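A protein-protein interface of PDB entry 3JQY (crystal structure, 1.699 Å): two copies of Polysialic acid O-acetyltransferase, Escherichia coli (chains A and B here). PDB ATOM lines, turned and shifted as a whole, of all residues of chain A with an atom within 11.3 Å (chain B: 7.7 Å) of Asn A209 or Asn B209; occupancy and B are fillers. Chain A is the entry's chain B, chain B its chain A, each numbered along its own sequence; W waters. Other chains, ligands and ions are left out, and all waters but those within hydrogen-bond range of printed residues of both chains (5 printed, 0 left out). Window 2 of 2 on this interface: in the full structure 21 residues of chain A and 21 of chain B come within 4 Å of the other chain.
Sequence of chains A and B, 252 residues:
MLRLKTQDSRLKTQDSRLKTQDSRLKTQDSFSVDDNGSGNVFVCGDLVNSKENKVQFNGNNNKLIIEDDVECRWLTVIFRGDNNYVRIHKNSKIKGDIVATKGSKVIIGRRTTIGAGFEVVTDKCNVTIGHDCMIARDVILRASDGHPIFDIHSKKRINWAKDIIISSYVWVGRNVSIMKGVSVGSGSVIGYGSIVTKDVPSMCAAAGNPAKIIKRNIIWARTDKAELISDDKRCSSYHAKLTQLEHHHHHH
The backbone carbonyl oxygen (O) of Asn A209 lies within hydrogen-bond range of the backbone NH (N) of Asn B209, 3.0 Å away.
The backbone carbonyl oxygen (O) of Gly B193 sits at hydrogen-bond distance from the side-chain amide nitrogen (ND2) of Asn A209.
The backbone NH (N) of Met A179 lies within hydrogen-bond range of the backbone carbonyl oxygen (O) of Val A196, 2.9 Å away.
The backbone NH (N) of Gly B193 sits close to the backbone carbonyl oxygen (O) of Asn B175 (3.3 Å).
The side-chain hydroxyl of Ser B194 lies within hydrogen-bond range of the backbone NH of Gly B208 (3.4 Å).
The backbone carbonyl oxygen (O) of Ser A177 is in hydrogen-bond range of the backbone NH (N) of Val A196.
N of Ile B195 is in hydrogen-bond range of O of Gly B208 (2.9 Å).
The backbone NH (N) of Ser A177 is in hydrogen-bond range of the backbone carbonyl oxygen (O) of Ser A194, at 3.0 Å.
Among the printed residues, pairs that only touch across the chains: Ser A177 with Tyr B192 (3.5 Å), Asn A209 with Gly B208 (3.6 Å), Ile A195 with Tyr B192 (3.7 Å), Met A179 with Tyr B192 (3.8 Å) and Ile A195 with Gly B193 (3.9 Å).
Of chain B, only Gly B193, Gly B208 and Asn B209 come within 4 Å of Asn A209.
Of chain A, only Asn A209 comes within 4 Å of Asn B209.
No residue of chain A comes within 4 Å of Ser B194.
No residue of chain A comes within 4 Å of Ala B207.
Printed residues of chain A within 4 Å of Gly B208: Asn A209.
No residue of chain A comes within 4 Å of Pro B210.
No residue of chain A comes within 4 Å of Ala B211.
Of the printed residues of chain B, Ser A177 touches Tyr B192 (3.5 Å).
Of the printed residues of chain B, Met A179 touches Tyr B192 (3.8 Å).
Of the printed residues of chain B, Ile A195 touches Tyr B192 and Gly B193.
Printed residues of chain A within 4 Å of Tyr B192: Ser A177 (3.5 Å), Met A179 (3.8 Å) and Ile A195 (3.7 Å).
Arg A174 touches none of the printed residues of chain B.
Thr B197 touches none of the printed residues of chain A.
The nearest residue of chain A that does not touch Asn B209 is Pro A210 (4.8 Å).
The nearest printed residue of chain B that does not touch Ile A195 is Ser B194 (5.3 Å).
Of the 25 printed residues of chain A, 4 touch a printed residue of chain B.
Hydrophobic or aromatic side chains of chain A that line the printed part of chain B: Met A179 and Ile A195.
Hydrophobic or aromatic side chains of chain B that line the printed part of chain A: Tyr B192.
Along chain B the printed residues that touch a printed residue of chain A span positions 192 to 209.
Among the printed residues, no Asp or Glu carboxylate lies within 4 Å of a Lys or Arg side-chain nitrogen of the other chain.
Met A179 touches Tyr B192, but with the chains exchanged Tyr A192 does not touch Met B179 (15.2 Å).
Ile A195 touches Tyr B192, but with the chains exchanged Tyr A192 does not touch Ile B195 (11.6 Å).
Asn A209 touches Gly B208, but with the chains exchanged Gly A208 does not touch Asn B209 (6.7 Å).
Asn A209 touches its own counterpart, Asn B209.
Of the 7 pairs that touch across the chains among the printed residues, 1 has its exchanged pair printed and touching as well.
Water W5 bridges the side-chain hydroxyl of Ser A177 (2.6 Å) and the side-chain hydroxyl of Tyr B192 (2.7 Å).
Water W4 lies within hydrogen-bond range of the backbone carbonyl oxygen (O) of Asn A209 (2.7 Å) and the backbone carbonyl oxygen (O) of Asn B209 (2.8 Å).
Water W1 bridges O of Gly B193 (2.7 Å) and ND2 of Asn A209 (3.5 Å).
Water W3 lies within hydrogen-bond range of the backbone carbonyl oxygen of Tyr B192 (2.8 Å), the backbone NH of Gly B208 (3.0 Å), the side-chain amide oxygen of Asn A209 (3.1 Å) and the backbone NH of Ser B194 (3.3 Å).
Water W2 bridges the side-chain amide nitrogen (ND2) of Asn B209 and the side-chain amide nitrogen (ND2) of Asn A209.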
ATOM      1  N   ARG A 174       6.424 -11.052 -11.138  1.00  0.00           N
ATOM      2  CA  ARG A 174       7.259 -12.159 -11.591  1.00  0.00           C
ATOM      3  C   ARG A 174       6.514 -13.117 -12.513  1.00  0.00           C
ATOM      4  O   ARG A 174       5.296 -13.289 -12.395  1.00  0.00           O
ATOM      5  CB  ARG A 174       7.807 -12.940 -10.391  1.00  0.00           C
ATOM      6  CG  ARG A 174       8.705 -14.099 -10.798  1.00  0.00           C
ATOM      7  CD  ARG A 174       9.488 -14.647  -9.618  1.00  0.00           C
ATOM      8  NE  ARG A 174      10.447 -15.665 -10.045  1.00  0.00           N
ATOM      9  CZ  ARG A 174      11.332 -16.243  -9.239  1.00  0.00           C
ATOM     10  NH1 ARG A 174      11.384 -15.905  -7.957  1.00  0.00           N
ATOM     11  NH2 ARG A 174      12.164 -17.162  -9.715  1.00  0.00           N
ATOM     12  N   ASN A 175       7.250 -13.738 -13.432  1.00  0.00           N
ATOM     13  CA  ASN A 175       6.670 -14.746 -14.315  1.00  0.00           C
ATOM     14  C   ASN A 175       5.491 -14.204 -15.120  1.00  0.00           C
ATOM     15  O   ASN A 175       4.413 -14.805 -15.135  1.00  0.00           O
ATOM     16  CB  ASN A 175       6.232 -15.967 -13.498  1.00  0.00           C
ATOM     17  CG  ASN A 175       5.894 -17.162 -14.365  1.00  0.00           C
ATOM     18  OD1 ASN A 175       6.417 -17.313 -15.472  1.00  0.00           O
ATOM     19  ND2 ASN A 175       5.018 -18.025 -13.864  1.00  0.00           N
ATOM     20  N   VAL A 176       5.707 -13.071 -15.783  1.00  0.00           N
ATOM     21  CA  VAL A 176       4.685 -12.410 -16.591  1.00  0.00           C
ATOM     22  C   VAL A 176       5.143 -12.350 -18.042  1.00  0.00           C
ATOM     23  O   VAL A 176       6.323 -12.138 -18.298  1.00  0.00           O
ATOM     24  CB  VAL A 176       4.464 -10.949 -16.105  1.00  0.00           C
ATOM     25  CG1 VAL A 176       3.743 -10.121 -17.179  1.00  0.00           C
ATOM     26  CG2 VAL A 176       3.709 -10.936 -14.785  1.00  0.00           C
ATOM     27  N   SER A 177       4.223 -12.544 -18.987  1.00  0.00           N
ATOM     28  CA  SER A 177       4.483 -12.211 -20.387  1.00  0.00           C
ATOM     29  C   SER A 177       3.569 -11.074 -20.811  1.00  0.00           C
ATOM     30  O   SER A 177       2.364 -11.104 -20.553  1.00  0.00           O
ATOM     31  CB  SER A 177       4.242 -13.403 -21.321  1.00  0.00           C
ATOM     32  OG  SER A 177       5.297 -14.344 -21.242  1.00  0.00           O
ATOM     33  N   ILE A 178       4.151 -10.070 -21.451  1.00  0.00           N
ATOM     34  CA  ILE A 178       3.375  -9.021 -22.090  1.00  0.00           C
ATOM     35  C   ILE A 178       3.458  -9.299 -23.584  1.00  0.00           C
ATOM     36  O   ILE A 178       4.550  -9.408 -24.140  1.00  0.00           O
ATOM     37  CB  ILE A 178       3.953  -7.633 -21.803  1.00  0.00           C
ATOM     38  CG1 ILE A 178       4.061  -7.391 -20.292  1.00  0.00           C
ATOM     39  CG2 ILE A 178       3.101  -6.552 -22.467  1.00  0.00           C
ATOM     40  CD1 ILE A 178       2.730  -7.317 -19.595  1.00  0.00           C
ATOM     41  N   MET A 179       2.304  -9.429 -24.231  1.00  0.00           N
ATOM     42  CA  MET A 179       2.258  -9.851 -25.621  1.00  0.00           C
ATOM     43  C   MET A 179       2.191  -8.640 -26.542  1.00  0.00           C
ATOM     44  O   MET A 179       2.156  -7.497 -26.083  1.00  0.00           O
ATOM     45  CB  MET A 179       1.068 -10.791 -25.868  1.00  0.00           C
ATOM     46  CG  MET A 179       1.128 -12.119 -25.103  1.00  0.00           C
ATOM     47  SD  MET A 179       2.737 -12.920 -25.207  1.00  0.00           S
ATOM     48  CE  MET A 179       2.330 -14.645 -24.931  1.00  0.00           C
ATOM     49  N   ILE A 190       1.058  -5.213 -12.804  1.00  0.00           N
ATOM     50  CA  ILE A 190       0.723  -6.474 -13.455  1.00  0.00           C
ATOM     51  C   ILE A 190       1.026  -7.609 -12.486  1.00  0.00           C
ATOM     52  O   ILE A 190       2.148  -7.735 -11.995  1.00  0.00           O
ATOM     53  CB  ILE A 190       1.530  -6.682 -14.752  1.00  0.00           C
ATOM     54  CG1 ILE A 190       1.330  -5.492 -15.694  1.00  0.00           C
ATOM     55  CG2 ILE A 190       1.125  -8.012 -15.417  1.00  0.00           C
ATOM     56  CD1 ILE A 190      -0.119  -5.283 -16.129  1.00  0.00           C
ATOM     57  N   GLY A 191       0.021  -8.430 -12.201  1.00  0.00           N
ATOM     58  CA  GLY A 191       0.165  -9.443 -11.177  1.00  0.00           C
ATOM     59  C   GLY A 191       1.032 -10.616 -11.587  1.00  0.00           C
ATOM     60  O   GLY A 191       1.161 -10.924 -12.770  1.00  0.00           O
ATOM     61  N   TYR A 192       1.626 -11.260 -10.589  1.00  0.00           N
ATOM     62  CA  TYR A 192       2.384 -12.492 -10.783  1.00  0.00           C
ATOM     63  C   TYR A 192       1.665 -13.446 -11.726  1.00  0.00           C
ATOM     64  O   TYR A 192       0.459 -13.674 -11.582  1.00  0.00           O
ATOM     65  CB  TYR A 192       2.581 -13.199  -9.434  1.00  0.00           C
ATOM     66  CG  TYR A 192       3.182 -14.577  -9.590  1.00  0.00           C
ATOM     67  CD1 TYR A 192       4.541 -14.789  -9.420  1.00  0.00           C
ATOM     68  CD2 TYR A 192       2.386 -15.665  -9.932  1.00  0.00           C
ATOM     69  CE1 TYR A 192       5.092 -16.053  -9.592  1.00  0.00           C
ATOM     70  CE2 TYR A 192       2.927 -16.923 -10.099  1.00  0.00           C
ATOM     71  CZ  TYR A 192       4.277 -17.112  -9.927  1.00  0.00           C
ATOM     72  OH  TYR A 192       4.815 -18.372 -10.092  1.00  0.00           O
ATOM     73  N   GLY A 193       2.405 -14.008 -12.682  1.00  0.00           N
ATOM     74  CA  GLY A 193       1.905 -15.087 -13.520  1.00  0.00           C
ATOM     75  C   GLY A 193       0.980 -14.694 -14.658  1.00  0.00           C
ATOM     76  O   GLY A 193       0.441 -15.555 -15.360  1.00  0.00           O
ATOM     77  N   SER A 194       0.797 -13.394 -14.850  1.00  0.00           N
ATOM     78  CA  SER A 194      -0.107 -12.886 -15.875  1.00  0.00           C
ATOM     79  C   SER A 194       0.409 -13.123 -17.283  1.00  0.00           C
ATOM     80  O   SER A 194       1.622 -13.153 -17.526  1.00  0.00           O
ATOM     81  CB  SER A 194      -0.332 -11.378 -15.696  1.00  0.00           C
ATOM     82  OG  SER A 194      -0.887 -11.069 -14.431  1.00  0.00           O
ATOM     83  N   ILE A 195      -0.520 -13.289 -18.219  1.00  0.00           N
ATOM     84  CA  ILE A 195      -0.203 -13.078 -19.625  1.00  0.00           C
ATOM     85  C   ILE A 195      -1.106 -11.954 -20.125  1.00  0.00           C
ATOM     86  O   ILE A 195      -2.332 -12.095 -20.165  1.00  0.00           O
ATOM     87  CB  ILE A 195      -0.378 -14.341 -20.469  1.00  0.00           C
ATOM     88  CG1 ILE A 195       0.569 -15.436 -19.966  1.00  0.00           C
ATOM     89  CG2 ILE A 195      -0.125 -14.018 -21.932  1.00  0.00           C
ATOM     90  CD1 ILE A 195       0.591 -16.695 -20.830  1.00  0.00           C
ATOM     91  N   VAL A 196      -0.490 -10.828 -20.469  1.00  0.00           N
ATOM     92  CA  VAL A 196      -1.215  -9.609 -20.815  1.00  0.00           C
ATOM     93  C   VAL A 196      -1.354  -9.479 -22.324  1.00  0.00           C
ATOM     94  O   VAL A 196      -0.355  -9.372 -23.041  1.00  0.00           O
ATOM     95  CB  VAL A 196      -0.491  -8.358 -20.255  1.00  0.00           C
ATOM     96  CG1 VAL A 196      -1.328  -7.116 -20.476  1.00  0.00           C
ATOM     97  CG2 VAL A 196      -0.177  -8.560 -18.783  1.00  0.00           C
ATOM     98  N   THR A 197      -2.594  -9.495 -22.806  1.00  0.00           N
ATOM     99  CA  THR A 197      -2.843  -9.495 -24.245  1.00  0.00           C
ATOM    100  C   THR A 197      -3.560  -8.243 -24.744  1.00  0.00           C
ATOM    101  O   THR A 197      -3.702  -8.052 -25.950  1.00  0.00           O
ATOM    102  CB  THR A 197      -3.674 -10.717 -24.665  1.00  0.00           C
ATOM    103  OG1 THR A 197      -4.971 -10.638 -24.061  1.00  0.00           O
ATOM    104  CG2 THR A 197      -2.986 -12.013 -24.233  1.00  0.00           C
ATOM    105  N   LYS A 198      -4.036  -7.414 -23.821  1.00  0.00           N
ATOM    106  CA  LYS A 198      -4.716  -6.173 -24.183  1.00  0.00           C
ATOM    107  C   LYS A 198      -4.183  -5.020 -23.338  1.00  0.00           C
ATOM    108  O   LYS A 198      -3.577  -5.244 -22.290  1.00  0.00           O
ATOM    109  CB  LYS A 198      -6.232  -6.320 -24.003  1.00  0.00           C
ATOM    110  CG  LYS A 198      -6.872  -7.270 -25.005  1.00  0.00           C
ATOM    111  CD  LYS A 198      -8.275  -7.676 -24.585  1.00  0.00           C
ATOM    112  CE  LYS A 198      -8.968  -8.463 -25.691  1.00  0.00           C
ATOM    113  NZ  LYS A 198      -8.078  -9.507 -26.276  1.00  0.00           N
ATOM    114  N   VAL A 200      -3.518  -2.098 -20.732  1.00  0.00           N
ATOM    115  CA  VAL A 200      -3.873  -1.870 -19.334  1.00  0.00           C
ATOM    116  C   VAL A 200      -3.796  -0.376 -19.054  1.00  0.00           C
ATOM    117  O   VAL A 200      -2.736   0.231 -19.197  1.00  0.00           O
ATOM    118  CB  VAL A 200      -2.924  -2.635 -18.385  1.00  0.00           C
ATOM    119  CG1 VAL A 200      -3.228  -2.302 -16.933  1.00  0.00           C
ATOM    120  CG2 VAL A 200      -3.016  -4.148 -18.643  1.00  0.00           C
ATOM    121  N   ALA A 206      -3.826  -5.439 -12.994  1.00  0.00           N
ATOM    122  CA  ALA A 206      -4.344  -6.459 -13.897  1.00  0.00           C
ATOM    123  C   ALA A 206      -3.666  -7.771 -13.573  1.00  0.00           C
ATOM    124  O   ALA A 206      -2.511  -7.781 -13.152  1.00  0.00           O
ATOM    125  CB  ALA A 206      -4.068  -6.078 -15.344  1.00  0.00           C
ATOM    126  N   ALA A 207      -4.386  -8.874 -13.761  1.00  0.00           N
ATOM    127  CA  ALA A 207      -3.827 -10.202 -13.538  1.00  0.00           C
ATOM    128  C   ALA A 207      -4.619 -11.261 -14.278  1.00  0.00           C
ATOM    129  O   ALA A 207      -5.768 -11.032 -14.662  1.00  0.00           O
ATOM    130  CB  ALA A 207      -3.789 -10.533 -12.059  1.00  0.00           C
ATOM    131  N   GLY A 208      -3.997 -12.420 -14.479  1.00  0.00           N
ATOM    132  CA  GLY A 208      -4.675 -13.548 -15.096  1.00  0.00           C
ATOM    133  C   GLY A 208      -4.044 -13.985 -16.407  1.00  0.00           C
ATOM    134  O   GLY A 208      -3.145 -13.336 -16.933  1.00  0.00           O
ATOM    135  N   ASN A 209      -4.528 -15.100 -16.938  1.00  0.00           N
ATOM    136  CA  ASN A 209      -4.116 -15.552 -18.258  1.00  0.00           C
ATOM    137  C   ASN A 209      -5.331 -16.021 -19.037  1.00  0.00           C
ATOM    138  O   ASN A 209      -5.780 -17.145 -18.851  1.00  0.00           O
ATOM    139  CB  ASN A 209      -3.112 -16.702 -18.148  1.00  0.00           C
ATOM    140  CG  ASN A 209      -2.764 -17.291 -19.515  1.00  0.00           C
ATOM    141  OD1 ASN A 209      -3.052 -16.683 -20.548  1.00  0.00           O
ATOM    142  ND2 ASN A 209      -2.160 -18.475 -19.523  1.00  0.00           N
ATOM    143  N   PRO A 210      -5.877 -15.162 -19.912  1.00  0.00           N
ATOM    144  CA  PRO A 210      -5.378 -13.818 -20.219  1.00  0.00           C
ATOM    145  C   PRO A 210      -5.723 -12.813 -19.132  1.00  0.00           C
ATOM    146  O   PRO A 210      -6.753 -12.947 -18.450  1.00  0.00           O
ATOM    147  CB  PRO A 210      -6.121 -13.464 -21.506  1.00  0.00           C
ATOM    148  CG  PRO A 210      -7.421 -14.191 -21.386  1.00  0.00           C
ATOM    149  CD  PRO A 210      -7.149 -15.451 -20.600  1.00  0.00           C
ATOM    150  N   ALA A 211      -4.874 -11.801 -18.971  1.00  0.00           N
ATOM    151  CA  ALA A 211      -5.052 -10.830 -17.902  1.00  0.00           C
ATOM    152  C   ALA A 211      -6.325 -10.012 -18.062  1.00  0.00           C
ATOM    153  O   ALA A 211      -6.766  -9.723 -19.177  1.00  0.00           O
ATOM    154  CB  ALA A 211      -3.828  -9.903 -17.791  1.00  0.00           C
ATOM    155  N   LYS A 212      -6.900  -9.644 -16.926  1.00  0.00           N
ATOM    156  CA  LYS A 212      -8.035  -8.726 -16.870  1.00  0.00           C
ATOM    157  C   LYS A 212      -7.803  -7.701 -15.765  1.00  0.00           C
ATOM    158  O   LYS A 212      -7.026  -7.939 -14.838  1.00  0.00           O
ATOM    159  CB  LYS A 212      -9.335  -9.493 -16.620  1.00  0.00           C
ATOM    160  CG  LYS A 212      -9.754 -10.373 -17.800  1.00  0.00           C
ATOM    161  CD  LYS A 212     -11.243 -10.662 -17.801  1.00  0.00           C
ATOM    162  CE  LYS A 212     -11.626 -11.633 -16.697  1.00  0.00           C
ATOM    163  NZ  LYS A 212     -12.974 -12.234 -16.936  1.00  0.00           N
ATOM    164  N   ILE A 213      -8.481  -6.559 -15.847  1.00  0.00           N
ATOM    165  CA  ILE A 213      -8.343  -5.543 -14.810  1.00  0.00           C
ATOM    166  C   ILE A 213      -9.039  -6.012 -13.545  1.00  0.00           C
ATOM    167  O   ILE A 213     -10.211  -6.393 -13.574  1.00  0.00           O
ATOM    168  CB  ILE A 213      -8.932  -4.192 -15.243  1.00  0.00           C
ATOM    169  CG1 ILE A 213      -8.201  -3.671 -16.482  1.00  0.00           C
ATOM    170  CG2 ILE A 213      -8.850  -3.194 -14.099  1.00  0.00           C
ATOM    171  CD1 ILE A 213      -8.844  -2.446 -17.107  1.00  0.00           C
ATOM    172  N   ILE A 214      -8.317  -6.007 -12.434  1.00  0.00           N
ATOM    173  CA  ILE A 214      -8.886  -6.495 -11.183  1.00  0.00           C
ATOM    174  C   ILE A 214      -9.153  -5.369 -10.187  1.00  0.00           C
ATOM    175  O   ILE A 214      -9.988  -5.512  -9.292  1.00  0.00           O
ATOM    176  CB  ILE A 214      -8.020  -7.602 -10.542  1.00  0.00           C
ATOM    177  CG1 ILE A 214      -6.626  -7.076 -10.212  1.00  0.00           C
ATOM    178  CG2 ILE A 214      -7.942  -8.817 -11.462  1.00  0.00           C
ATOM    179  CD1 ILE A 214      -5.741  -8.086  -9.500  1.00  0.00           C
ATOM    180  N   ASN B 175       5.811 -23.479 -23.279  1.00  0.00           N
ATOM    181  CA  ASN B 175       5.252 -23.472 -21.965  1.00  0.00           C
ATOM    182  C   ASN B 175       3.755 -23.749 -21.956  1.00  0.00           C
ATOM    183  O   ASN B 175       3.028 -23.026 -21.384  1.00  0.00           O
ATOM    184  CB  ASN B 175       5.544 -22.161 -21.238  1.00  0.00           C
ATOM    185  CG  ASN B 175       5.241 -22.226 -19.775  1.00  0.00           C
ATOM    186  OD1 ASN B 175       5.235 -23.268 -19.184  1.00  0.00           O
ATOM    187  ND2 ASN B 175       4.993 -21.071 -19.184  1.00  0.00           N
ATOM    188  N   MET B 179      -4.015 -31.197 -21.624  1.00  0.00           N
ATOM    189  CA  MET B 179      -4.548 -32.139 -20.634  1.00  0.00           C
ATOM    190  C   MET B 179      -5.321 -33.301 -21.259  1.00  0.00           C
ATOM    191  O   MET B 179      -5.456 -33.385 -22.479  1.00  0.00           O
ATOM    192  CB  MET B 179      -5.416 -31.400 -19.609  1.00  0.00           C
ATOM    193  CG  MET B 179      -4.683 -30.290 -18.856  1.00  0.00           C
ATOM    194  SD  MET B 179      -3.114 -30.852 -18.144  1.00  0.00           S
ATOM    195  CE  MET B 179      -2.832 -29.589 -16.901  1.00  0.00           C
ATOM    196  N   GLY B 191      -1.302 -21.142 -28.193  1.00  0.00           N
ATOM    197  CA  GLY B 191      -0.474 -20.023 -27.780  1.00  0.00           C
ATOM    198  C   GLY B 191       0.397 -20.290 -26.576  1.00  0.00           C
ATOM    199  O   GLY B 191       0.060 -21.110 -25.712  1.00  0.00           O
ATOM    200  N   TYR B 192       1.523 -19.582 -26.516  1.00  0.00           N
ATOM    201  CA  TYR B 192       2.407 -19.602 -25.354  1.00  0.00           C
ATOM    202  C   TYR B 192       1.614 -19.602 -24.059  1.00  0.00           C
ATOM    203  O   TYR B 192       0.657 -18.833 -23.916  1.00  0.00           O
ATOM    204  CB  TYR B 192       3.309 -18.357 -25.344  1.00  0.00           C
ATOM    205  CG  TYR B 192       4.080 -18.236 -24.049  1.00  0.00           C
ATOM    206  CD1 TYR B 192       5.378 -18.716 -23.944  1.00  0.00           C
ATOM    207  CD2 TYR B 192       3.489 -17.688 -22.919  1.00  0.00           C
ATOM    208  CE1 TYR B 192       6.077 -18.638 -22.749  1.00  0.00           C
ATOM    209  CE2 TYR B 192       4.175 -17.607 -21.722  1.00  0.00           C
ATOM    210  CZ  TYR B 192       5.464 -18.087 -21.642  1.00  0.00           C
ATOM    211  OH  TYR B 192       6.145 -18.003 -20.451  1.00  0.00           O
ATOM    212  N   GLY B 193       2.012 -20.454 -23.115  1.00  0.00           N
ATOM    213  CA  GLY B 193       1.497 -20.378 -21.757  1.00  0.00           C
ATOM    214  C   GLY B 193       0.143 -21.036 -21.551  1.00  0.00           C
ATOM    215  O   GLY B 193      -0.400 -21.019 -20.445  1.00  0.00           O
ATOM    216  N   SER B 194      -0.409 -21.618 -22.607  1.00  0.00           N
ATOM    217  CA  SER B 194      -1.754 -22.183 -22.508  1.00  0.00           C
ATOM    218  C   SER B 194      -1.817 -23.424 -21.621  1.00  0.00           C
ATOM    219  O   SER B 194      -0.849 -24.167 -21.506  1.00  0.00           O
ATOM    220  CB  SER B 194      -2.276 -22.549 -23.901  1.00  0.00           C
ATOM    221  OG  SER B 194      -2.406 -21.388 -24.706  1.00  0.00           O
ATOM    222  N   ILE B 195      -2.974 -23.641 -21.002  1.00  0.00           N
ATOM    223  CA  ILE B 195      -3.338 -24.968 -20.519  1.00  0.00           C
ATOM    224  C   ILE B 195      -4.633 -25.343 -21.223  1.00  0.00           C
ATOM    225  O   ILE B 195      -5.675 -24.727 -21.007  1.00  0.00           O
ATOM    226  CB  ILE B 195      -3.492 -25.042 -18.983  1.00  0.00           C
ATOM    227  CG1 ILE B 195      -2.154 -24.708 -18.311  1.00  0.00           C
ATOM    228  CG2 ILE B 195      -3.975 -26.435 -18.579  1.00  0.00           C
ATOM    229  CD1 ILE B 195      -2.112 -24.935 -16.797  1.00  0.00           C
ATOM    230  N   VAL B 196      -4.541 -26.334 -22.103  1.00  0.00           N
ATOM    231  CA  VAL B 196      -5.652 -26.725 -22.960  1.00  0.00           C
ATOM    232  C   VAL B 196      -6.395 -27.895 -22.334  1.00  0.00           C
ATOM    233  O   VAL B 196      -5.811 -28.960 -22.100  1.00  0.00           O
ATOM    234  CB  VAL B 196      -5.154 -27.132 -24.358  1.00  0.00           C
ATOM    235  CG1 VAL B 196      -6.339 -27.469 -25.259  1.00  0.00           C
ATOM    236  CG2 VAL B 196      -4.292 -26.024 -24.968  1.00  0.00           C
ATOM    237  N   THR B 197      -7.682 -27.699 -22.060  1.00  0.00           N
ATOM    238  CA  THR B 197      -8.469 -28.716 -21.367  1.00  0.00           C
ATOM    239  C   THR B 197      -9.635 -29.244 -22.201  1.00  0.00           C
ATOM    240  O   THR B 197     -10.251 -30.240 -21.829  1.00  0.00           O
ATOM    241  CB  THR B 197      -9.024 -28.177 -20.028  1.00  0.00           C
ATOM    242  OG1 THR B 197      -9.876 -27.054 -20.283  1.00  0.00           O
ATOM    243  CG2 THR B 197      -7.888 -27.736 -19.119  1.00  0.00           C
ATOM    244  N   ALA B 207      -5.659 -19.975 -26.817  1.00  0.00           N
ATOM    245  CA  ALA B 207      -4.732 -19.549 -25.778  1.00  0.00           C
ATOM    246  C   ALA B 207      -5.463 -19.305 -24.464  1.00  0.00           C
ATOM    247  O   ALA B 207      -6.679 -19.116 -24.447  1.00  0.00           O
ATOM    248  CB  ALA B 207      -3.967 -18.282 -26.210  1.00  0.00           C
ATOM    249  N   GLY B 208      -4.711 -19.307 -23.364  1.00  0.00           N
ATOM    250  CA  GLY B 208      -5.274 -19.044 -22.052  1.00  0.00           C
ATOM    251  C   GLY B 208      -5.126 -20.201 -21.081  1.00  0.00           C
ATOM    252  O   GLY B 208      -4.679 -21.291 -21.448  1.00  0.00           O
ATOM    253  N   ASN B 209      -5.501 -19.951 -19.832  1.00  0.00           N
ATOM    254  CA  ASN B 209      -5.548 -20.985 -18.808  1.00  0.00           C
ATOM    255  C   ASN B 209      -6.817 -20.798 -17.990  1.00  0.00           C
ATOM    256  O   ASN B 209      -6.842 -19.985 -17.068  1.00  0.00           O
ATOM    257  CB  ASN B 209      -4.335 -20.884 -17.879  1.00  0.00           C
ATOM    258  CG  ASN B 209      -4.397 -21.893 -16.737  1.00  0.00           C
ATOM    259  OD1 ASN B 209      -5.208 -22.815 -16.768  1.00  0.00           O
ATOM    260  ND2 ASN B 209      -3.521 -21.739 -15.743  1.00  0.00           N
ATOM    261  N   PRO B 210      -7.885 -21.534 -18.338  1.00  0.00           N
ATOM    262  CA  PRO B 210      -7.908 -22.538 -19.413  1.00  0.00           C
ATOM    263  C   PRO B 210      -7.976 -21.906 -20.800  1.00  0.00           C
ATOM    264  O   PRO B 210      -8.480 -20.793 -20.965  1.00  0.00           O
ATOM    265  CB  PRO B 210      -9.197 -23.304 -19.135  1.00  0.00           C
ATOM    266  CG  PRO B 210     -10.091 -22.302 -18.496  1.00  0.00           C
ATOM    267  CD  PRO B 210      -9.205 -21.357 -17.712  1.00  0.00           C
ATOM    268  N   ALA B 211      -7.482 -22.626 -21.803  1.00  0.00           N
ATOM    269  CA  ALA B 211      -7.418 -22.086 -23.149  1.00  0.00           C
ATOM    270  C   ALA B 211      -8.811 -21.933 -23.757  1.00  0.00           C
ATOM    271  O   ALA B 211      -9.727 -22.719 -23.471  1.00  0.00           O
ATOM    272  CB  ALA B 211      -6.529 -22.967 -24.032  1.00  0.00           C
ATOM    273  N   LYS B 212      -8.966 -20.891 -24.566  1.00  0.00           N
ATOM    274  CA  LYS B 212     -10.190 -20.666 -25.314  1.00  0.00           C
ATOM    275  C   LYS B 212      -9.787 -20.371 -26.744  1.00  0.00           C
ATOM    276  O   LYS B 212      -8.670 -19.920 -26.994  1.00  0.00           O
ATOM    277  CB  LYS B 212     -10.957 -19.470 -24.752  1.00  0.00           C
ATOM    278  CG  LYS B 212     -11.188 -19.526 -23.254  1.00  0.00           C
ATOM    279  CD  LYS B 212     -12.015 -20.740 -22.875  1.00  0.00           C
ATOM    280  CE  LYS B 212     -12.452 -20.668 -21.421  1.00  0.00           C
ATOM    281  NZ  LYS B 212     -13.041 -19.335 -21.108  1.00  0.00           N
HETATM  282  O   HOH W   1       0.805 -19.843 -18.292  1.00  0.00           O
HETATM  283  O   HOH W   2      -1.372 -19.347 -16.384  1.00  0.00           O
HETATM  284  O   HOH W   3      -1.857 -18.696 -22.654  1.00  0.00           O
HETATM  285  O   HOH W   4      -8.052 -17.506 -17.422  1.00  0.00           O
HETATM  286  O   HOH W   5       5.439 -15.770 -19.059  1.00  0.00           O
